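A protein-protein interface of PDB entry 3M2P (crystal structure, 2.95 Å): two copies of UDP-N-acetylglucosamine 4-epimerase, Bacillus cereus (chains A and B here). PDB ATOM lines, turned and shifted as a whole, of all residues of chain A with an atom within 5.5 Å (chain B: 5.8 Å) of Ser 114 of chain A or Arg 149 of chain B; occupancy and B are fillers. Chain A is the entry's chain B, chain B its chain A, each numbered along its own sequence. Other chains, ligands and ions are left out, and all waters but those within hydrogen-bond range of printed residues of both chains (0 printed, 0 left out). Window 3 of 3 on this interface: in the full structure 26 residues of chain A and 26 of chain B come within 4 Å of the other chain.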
ATOM      1  N   ILE A 110     -19.929 -19.678  17.212  1.00  0.00           N
ATOM      2  CA  ILE A 110     -19.924 -21.131  17.062  1.00  0.00           C
ATOM      3  C   ILE A 110     -20.483 -21.830  18.289  1.00  0.00           C
ATOM      4  O   ILE A 110     -20.888 -22.992  18.226  1.00  0.00           O
ATOM      5  CB  ILE A 110     -18.497 -21.648  16.902  1.00  0.00           C
ATOM      6  CG1 ILE A 110     -18.493 -23.158  16.633  1.00  0.00           C
ATOM      7  CG2 ILE A 110     -17.701 -21.335  18.142  1.00  0.00           C
ATOM      8  CD1 ILE A 110     -17.117 -23.719  16.307  1.00  0.00           C
ATOM      9  N   ALA A 112     -23.147 -21.627  19.437  1.00  0.00           N
ATOM     10  CA  ALA A 112     -24.553 -21.952  19.216  1.00  0.00           C
ATOM     11  C   ALA A 112     -24.699 -23.460  19.091  1.00  0.00           C
ATOM     12  O   ALA A 112     -25.743 -24.028  19.397  1.00  0.00           O
ATOM     13  CB  ALA A 112     -25.072 -21.271  17.961  1.00  0.00           C
ATOM     14  N   TYR A 113     -23.630 -24.106  18.652  1.00  0.00           N
ATOM     15  CA  TYR A 113     -23.654 -25.529  18.433  1.00  0.00           C
ATOM     16  C   TYR A 113     -23.056 -26.277  19.621  1.00  0.00           C
ATOM     17  O   TYR A 113     -22.424 -25.673  20.493  1.00  0.00           O
ATOM     18  CB  TYR A 113     -22.866 -25.860  17.171  1.00  0.00           C
ATOM     19  CG  TYR A 113     -23.232 -25.056  15.936  1.00  0.00           C
ATOM     20  CD1 TYR A 113     -24.505 -25.095  15.401  1.00  0.00           C
ATOM     21  CD2 TYR A 113     -22.281 -24.297  15.282  1.00  0.00           C
ATOM     22  CE1 TYR A 113     -24.821 -24.373  14.266  1.00  0.00           C
ATOM     23  CE2 TYR A 113     -22.584 -23.578  14.150  1.00  0.00           C
ATOM     24  CZ  TYR A 113     -23.850 -23.613  13.643  1.00  0.00           C
ATOM     25  OH  TYR A 113     -24.141 -22.879  12.511  1.00  0.00           O
ATOM     26  N   SER A 114     -23.249 -27.596  19.656  1.00  0.00           N
ATOM     27  CA  SER A 114     -22.592 -28.421  20.678  1.00  0.00           C
ATOM     28  C   SER A 114     -22.519 -29.924  20.375  1.00  0.00           C
ATOM     29  O   SER A 114     -21.558 -30.578  20.762  1.00  0.00           O
ATOM     30  CB  SER A 114     -23.194 -28.179  22.072  1.00  0.00           C
ATOM     31  OG  SER A 114     -24.524 -28.649  22.158  1.00  0.00           O
ATOM     32  N   ASP A 115     -23.517 -30.467  19.688  1.00  0.00           N
ATOM     33  CA  ASP A 115     -23.599 -31.911  19.451  1.00  0.00           C
ATOM     34  C   ASP A 115     -22.490 -32.452  18.546  1.00  0.00           C
ATOM     35  O   ASP A 115     -22.561 -32.330  17.324  1.00  0.00           O
ATOM     36  CB  ASP A 115     -24.970 -32.270  18.871  1.00  0.00           C
ATOM     37  CG  ASP A 115     -25.104 -33.743  18.544  1.00  0.00           C
ATOM     38  OD1 ASP A 115     -24.119 -34.497  18.731  1.00  0.00           O
ATOM     39  OD2 ASP A 115     -26.204 -34.147  18.101  1.00  0.00           O
ATOM     40  N   GLU A 116     -21.486 -33.081  19.160  1.00  0.00           N
ATOM     41  CA  GLU A 116     -20.314 -33.628  18.449  1.00  0.00           C
ATOM     42  C   GLU A 116     -20.693 -34.584  17.304  1.00  0.00           C
ATOM     43  O   GLU A 116     -19.958 -34.756  16.329  1.00  0.00           O
ATOM     44  CB  GLU A 116     -19.359 -34.313  19.449  1.00  0.00           C
ATOM     45  CG  GLU A 116     -18.503 -33.317  20.254  1.00  0.00           C
ATOM     46  CD  GLU A 116     -17.777 -33.926  21.471  1.00  0.00           C
ATOM     47  OE1 GLU A 116     -18.238 -34.956  22.024  1.00  0.00           O
ATOM     48  OE2 GLU A 116     -16.742 -33.350  21.887  1.00  0.00           O
ATOM     49  N   TRP A 121     -20.475 -28.677  11.764  1.00  0.00           N
ATOM     50  CA  TRP A 121     -21.760 -28.016  11.911  1.00  0.00           C
ATOM     51  C   TRP A 121     -22.029 -27.025  10.803  1.00  0.00           C
ATOM     52  O   TRP A 121     -21.228 -26.125  10.559  1.00  0.00           O
ATOM     53  CB  TRP A 121     -21.815 -27.274  13.221  1.00  0.00           C
ATOM     54  CG  TRP A 121     -21.748 -28.152  14.387  1.00  0.00           C
ATOM     55  CD1 TRP A 121     -22.405 -29.330  14.560  1.00  0.00           C
ATOM     56  CD2 TRP A 121     -21.013 -27.913  15.587  1.00  0.00           C
ATOM     57  NE1 TRP A 121     -22.110 -29.851  15.794  1.00  0.00           N
ATOM     58  CE2 TRP A 121     -21.259 -28.994  16.447  1.00  0.00           C
ATOM     59  CE3 TRP A 121     -20.171 -26.890  16.018  1.00  0.00           C
ATOM     60  CZ2 TRP A 121     -20.693 -29.081  17.713  1.00  0.00           C
ATOM     61  CZ3 TRP A 121     -19.608 -26.980  17.276  1.00  0.00           C
ATOM     62  CH2 TRP A 121     -19.870 -28.065  18.106  1.00  0.00           C
ATOM     63  N   LEU A 128     -27.728 -25.881  19.879  1.00  0.00           N
ATOM     64  CA  LEU A 128     -27.748 -26.573  21.158  1.00  0.00           C
ATOM     65  C   LEU A 128     -26.729 -25.917  22.088  1.00  0.00           C
ATOM     66  O   LEU A 128     -25.667 -26.479  22.351  1.00  0.00           O
ATOM     67  CB  LEU A 128     -27.444 -28.059  20.957  1.00  0.00           C
ATOM     68  CG  LEU A 128     -27.722 -29.011  22.116  1.00  0.00           C
ATOM     69  CD1 LEU A 128     -29.200 -29.204  22.312  1.00  0.00           C
ATOM     70  CD2 LEU A 128     -27.045 -30.333  21.880  1.00  0.00           C
ATOM     71  N   PRO A 129     -27.056 -24.718  22.590  1.00  0.00           N
ATOM     72  CA  PRO A 129     -26.093 -23.958  23.394  1.00  0.00           C
ATOM     73  C   PRO A 129     -25.640 -24.754  24.626  1.00  0.00           C
ATOM     74  O   PRO A 129     -26.417 -25.491  25.227  1.00  0.00           O
ATOM     75  CB  PRO A 129     -26.883 -22.711  23.816  1.00  0.00           C
ATOM     76  CG  PRO A 129     -28.084 -22.678  22.942  1.00  0.00           C
ATOM     77  CD  PRO A 129     -28.387 -24.093  22.583  1.00  0.00           C
ATOM     78  N   ASP A 130     -24.372 -24.600  24.979  1.00  0.00           N
ATOM     79  CA  ASP A 130     -23.790 -25.330  26.092  1.00  0.00           C
ATOM     80  C   ASP A 130     -23.626 -24.396  27.281  1.00  0.00           C
ATOM     81  O   ASP A 130     -23.419 -24.842  28.411  1.00  0.00           O
ATOM     82  CB  ASP A 130     -22.428 -25.892  25.686  1.00  0.00           C
ATOM     83  CG  ASP A 130     -22.169 -27.270  26.268  1.00  0.00           C
ATOM     84  OD1 ASP A 130     -23.121 -28.088  26.316  1.00  0.00           O
ATOM     85  OD2 ASP A 130     -21.008 -27.535  26.663  1.00  0.00           O
ATOM     86  N   SER A 262     -14.953 -31.211  21.001  1.00  0.00           N
ATOM     87  CA  SER A 262     -14.666 -30.855  19.616  1.00  0.00           C
ATOM     88  C   SER A 262     -15.680 -29.857  19.029  1.00  0.00           C
ATOM     89  O   SER A 262     -16.898 -29.997  19.209  1.00  0.00           O
ATOM     90  CB  SER A 262     -14.576 -32.114  18.744  1.00  0.00           C
ATOM     91  OG  SER A 262     -13.253 -32.626  18.707  1.00  0.00           O
ATOM     92  N   HIS B 142     -33.563 -24.230  26.144  1.00  0.00           N
ATOM     93  CA  HIS B 142     -32.141 -24.514  26.232  1.00  0.00           C
ATOM     94  C   HIS B 142     -31.570 -24.349  27.644  1.00  0.00           C
ATOM     95  O   HIS B 142     -30.597 -25.015  28.010  1.00  0.00           O
ATOM     96  CB  HIS B 142     -31.382 -23.694  25.199  1.00  0.00           C
ATOM     97  CG  HIS B 142     -31.640 -24.146  23.800  1.00  0.00           C
ATOM     98  ND1 HIS B 142     -31.051 -25.272  23.264  1.00  0.00           N
ATOM     99  CD2 HIS B 142     -32.457 -23.655  22.837  1.00  0.00           C
ATOM    100  CE1 HIS B 142     -31.476 -25.441  22.024  1.00  0.00           C
ATOM    101  NE2 HIS B 142     -32.332 -24.476  21.743  1.00  0.00           N
ATOM    102  N   GLY B 144     -33.187 -25.418  30.248  1.00  0.00           N
ATOM    103  CA  GLY B 144     -33.451 -26.767  30.706  1.00  0.00           C
ATOM    104  C   GLY B 144     -32.500 -27.763  30.073  1.00  0.00           C
ATOM    105  O   GLY B 144     -31.971 -28.627  30.761  1.00  0.00           O
ATOM    106  N   ASN B 145     -32.291 -27.641  28.763  1.00  0.00           N
ATOM    107  CA  ASN B 145     -31.394 -28.522  28.027  1.00  0.00           C
ATOM    108  C   ASN B 145     -30.045 -28.571  28.699  1.00  0.00           C
ATOM    109  O   ASN B 145     -29.481 -29.639  28.931  1.00  0.00           O
ATOM    110  CB  ASN B 145     -31.187 -28.021  26.603  1.00  0.00           C
ATOM    111  CG  ASN B 145     -32.410 -28.200  25.735  1.00  0.00           C
ATOM    112  OD1 ASN B 145     -32.462 -27.694  24.611  1.00  0.00           O
ATOM    113  ND2 ASN B 145     -33.400 -28.914  26.246  1.00  0.00           N
ATOM    114  N   ILE B 146     -29.519 -27.398  29.010  1.00  0.00           N
ATOM    115  CA  ILE B 146     -28.209 -27.325  29.632  1.00  0.00           C
ATOM    116  C   ILE B 146     -28.184 -27.999  31.016  1.00  0.00           C
ATOM    117  O   ILE B 146     -27.301 -28.806  31.307  1.00  0.00           O
ATOM    118  CB  ILE B 146     -27.690 -25.886  29.660  1.00  0.00           C
ATOM    119  CG1 ILE B 146     -27.123 -25.534  28.283  1.00  0.00           C
ATOM    120  CG2 ILE B 146     -26.630 -25.731  30.728  1.00  0.00           C
ATOM    121  CD1 ILE B 146     -27.214 -24.089  27.915  1.00  0.00           C
ATOM    122  N   TYR B 147     -29.170 -27.702  31.853  1.00  0.00           N
ATOM    123  CA  TYR B 147     -29.274 -28.379  33.139  1.00  0.00           C
ATOM    124  C   TYR B 147     -29.445 -29.881  32.982  1.00  0.00           C
ATOM    125  O   TYR B 147     -29.070 -30.649  33.863  1.00  0.00           O
ATOM    126  CB  TYR B 147     -30.428 -27.810  33.961  1.00  0.00           C
ATOM    127  CG  TYR B 147     -30.047 -26.572  34.717  1.00  0.00           C
ATOM    128  CD1 TYR B 147     -29.641 -25.441  34.049  1.00  0.00           C
ATOM    129  CD2 TYR B 147     -30.071 -26.545  36.101  1.00  0.00           C
ATOM    130  CE1 TYR B 147     -29.281 -24.314  34.725  1.00  0.00           C
ATOM    131  CE2 TYR B 147     -29.711 -25.418  36.789  1.00  0.00           C
ATOM    132  CZ  TYR B 147     -29.317 -24.300  36.092  1.00  0.00           C
ATOM    133  OH  TYR B 147     -28.957 -23.149  36.756  1.00  0.00           O
ATOM    134  N   SER B 148     -30.020 -30.305  31.864  1.00  0.00           N
ATOM    135  CA  SER B 148     -30.268 -31.730  31.656  1.00  0.00           C
ATOM    136  C   SER B 148     -28.988 -32.471  31.308  1.00  0.00           C
ATOM    137  O   SER B 148     -28.710 -33.539  31.848  1.00  0.00           O
ATOM    138  CB  SER B 148     -31.342 -31.956  30.591  1.00  0.00           C
ATOM    139  OG  SER B 148     -32.638 -31.783  31.144  1.00  0.00           O
ATOM    140  N   ARG B 149     -28.202 -31.877  30.417  1.00  0.00           N
ATOM    141  CA  ARG B 149     -26.940 -32.471  30.004  1.00  0.00           C
ATOM    142  C   ARG B 149     -25.864 -32.339  31.068  1.00  0.00           C
ATOM    143  O   ARG B 149     -25.018 -33.206  31.192  1.00  0.00           O
ATOM    144  CB  ARG B 149     -26.477 -31.886  28.665  1.00  0.00           C
ATOM    145  CG  ARG B 149     -27.521 -32.064  27.557  1.00  0.00           C
ATOM    146  CD  ARG B 149     -26.970 -31.783  26.160  1.00  0.00           C
ATOM    147  NE  ARG B 149     -26.170 -30.560  26.083  1.00  0.00           N
ATOM    148  CZ  ARG B 149     -26.657 -29.347  25.827  1.00  0.00           C
ATOM    149  NH1 ARG B 149     -27.951 -29.163  25.627  1.00  0.00           N
ATOM    150  NH2 ARG B 149     -25.838 -28.311  25.771  1.00  0.00           N
ATOM    151  N   LYS B 150     -25.919 -31.276  31.861  1.00  0.00           N
ATOM    152  CA  LYS B 150     -24.825 -30.953  32.775  1.00  0.00           C
ATOM    153  C   LYS B 150     -25.167 -31.124  34.252  1.00  0.00           C
ATOM    154  O   LYS B 150     -24.271 -31.171  35.100  1.00  0.00           O
ATOM    155  CB  LYS B 150     -24.317 -29.530  32.519  1.00  0.00           C
ATOM    156  CG  LYS B 150     -23.855 -29.315  31.099  1.00  0.00           C
ATOM    157  CD  LYS B 150     -22.959 -28.105  30.964  1.00  0.00           C
ATOM    158  CE  LYS B 150     -22.318 -28.072  29.573  1.00  0.00           C
ATOM    159  NZ  LYS B 150     -21.779 -29.420  29.159  1.00  0.00           N
ATOM    160  N   LYS B 151     -26.451 -31.219  34.568  1.00  0.00           N
ATOM    161  CA  LYS B 151     -26.858 -31.391  35.954  1.00  0.00           C
ATOM    162  C   LYS B 151     -27.659 -32.680  36.129  1.00  0.00           C
ATOM    163  O   LYS B 151     -28.254 -32.919  37.189  1.00  0.00           O
ATOM    164  CB  LYS B 151     -27.664 -30.180  36.441  1.00  0.00           C
ATOM    165  CG  LYS B 151     -26.911 -28.856  36.398  1.00  0.00           C
ATOM    166  CD  LYS B 151     -25.751 -28.858  37.390  1.00  0.00           C
ATOM    167  CE  LYS B 151     -24.772 -27.735  37.092  1.00  0.00           C
ATOM    168  NZ  LYS B 151     -25.434 -26.388  37.135  1.00  0.00           N
ATOM    169  N   GLY B 152     -27.669 -33.518  35.097  1.00  0.00           N
ATOM    170  CA  GLY B 152     -28.410 -34.758  35.168  1.00  0.00           C
ATOM    171  C   GLY B 152     -29.844 -34.492  35.584  1.00  0.00           C
ATOM    172  O   GLY B 152     -30.498 -35.324  36.206  1.00  0.00           O
ATOM    173  N   LEU B 153     -30.333 -33.305  35.257  1.00  0.00           N
ATOM    174  CA  LEU B 153     -31.731 -32.991  35.475  1.00  0.00           C
ATOM    175  C   LEU B 153     -32.498 -33.607  34.307  1.00  0.00           C
ATOM    176  O   LEU B 153     -31.927 -33.792  33.235  1.00  0.00           O
ATOM    177  CB  LEU B 153     -31.909 -31.481  35.537  1.00  0.00           C
ATOM    178  CG  LEU B 153     -32.656 -31.046  36.795  1.00  0.00           C
ATOM    179  CD1 LEU B 153     -31.841 -31.422  38.022  1.00  0.00           C
ATOM    180  CD2 LEU B 153     -32.979 -29.561  36.761  1.00  0.00           C
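The side-chain carboxylate (OD2) of Asp 130 of chain A lies within salt-bridge range of the side-chain amino group (NZ) of Lys 150 of chain B, at 3.2 Å.
NH2 of Arg 149 of chain B lies within salt-bridge range of OD1 of Asp 130 of chain A, 2.8 Å away.
The backbone carbonyl oxygen of Pro 129 of chain A sits at hydrogen-bond distance from the guanidinium group of Arg 149 of chain B.
ND1 of His 142 of chain B is in hydrogen-bond range of OD1 of Asn 145 of chain B (3.1 Å).
OG of Ser 114 of chain A is in hydrogen-bond range of O of Leu 128 of chain A, at 2.5 Å.
The backbone carbonyl oxygen (O) of Ala 112 of chain A lies within hydrogen-bond range of the backbone NH (N) of Leu 128 of chain A (2.8 Å).
Among the printed residues, merely in contact across the chains: Pro 129 of chain A with His 142 of chain B (3.0 Å), Pro 129 of chain A with Ile 146 of chain B (3.1 Å), Leu 128 of chain A with Arg 149 of chain B (3.5 Å), Asp 130 of chain A with Ile 146 of chain B (3.7 Å), Ser 114 of chain A with Arg 149 of chain B (3.9 Å) and Leu 128 of chain A with His 142 of chain B (3.99 Å).
Of chain B, only Arg 149 (3.9 Å) comes within 4 Å of Ser 114 of chain A.
Of the printed residues of chain B, Leu 128 of chain A touches His 142 (3.99 Å) and Arg 149 (3.5 Å).
Of the printed residues of chain B, Pro 129 of chain A touches His 142, Ile 146 and Arg 149.
Printed residues of chain A within 4 Å of His 142 of chain B: Leu 128 and Pro 129.
Printed residues of chain A within 4 Å of Ile 146 of chain B: Pro 129 and Asp 130.
Of chain A, only Ser 114, Leu 128, Pro 129 and Asp 130 come within 4 Å of Arg 149 of chain B.
Printed residues of chain A within 4 Å of Lys 150 of chain B: Asp 130.
The nearest printed residue of chain A that does not touch Arg 149 of chain B is Tyr 113 of chain A (6.8 Å).
Hydrophobic or aromatic side chains of chain B that line the printed part of chain A: His 142 and Ile 146.
No position is printed for both chains.
Of the 9 pairs that touch across the chains among the printed residues, none has its exchanged pair printed and touching as well.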
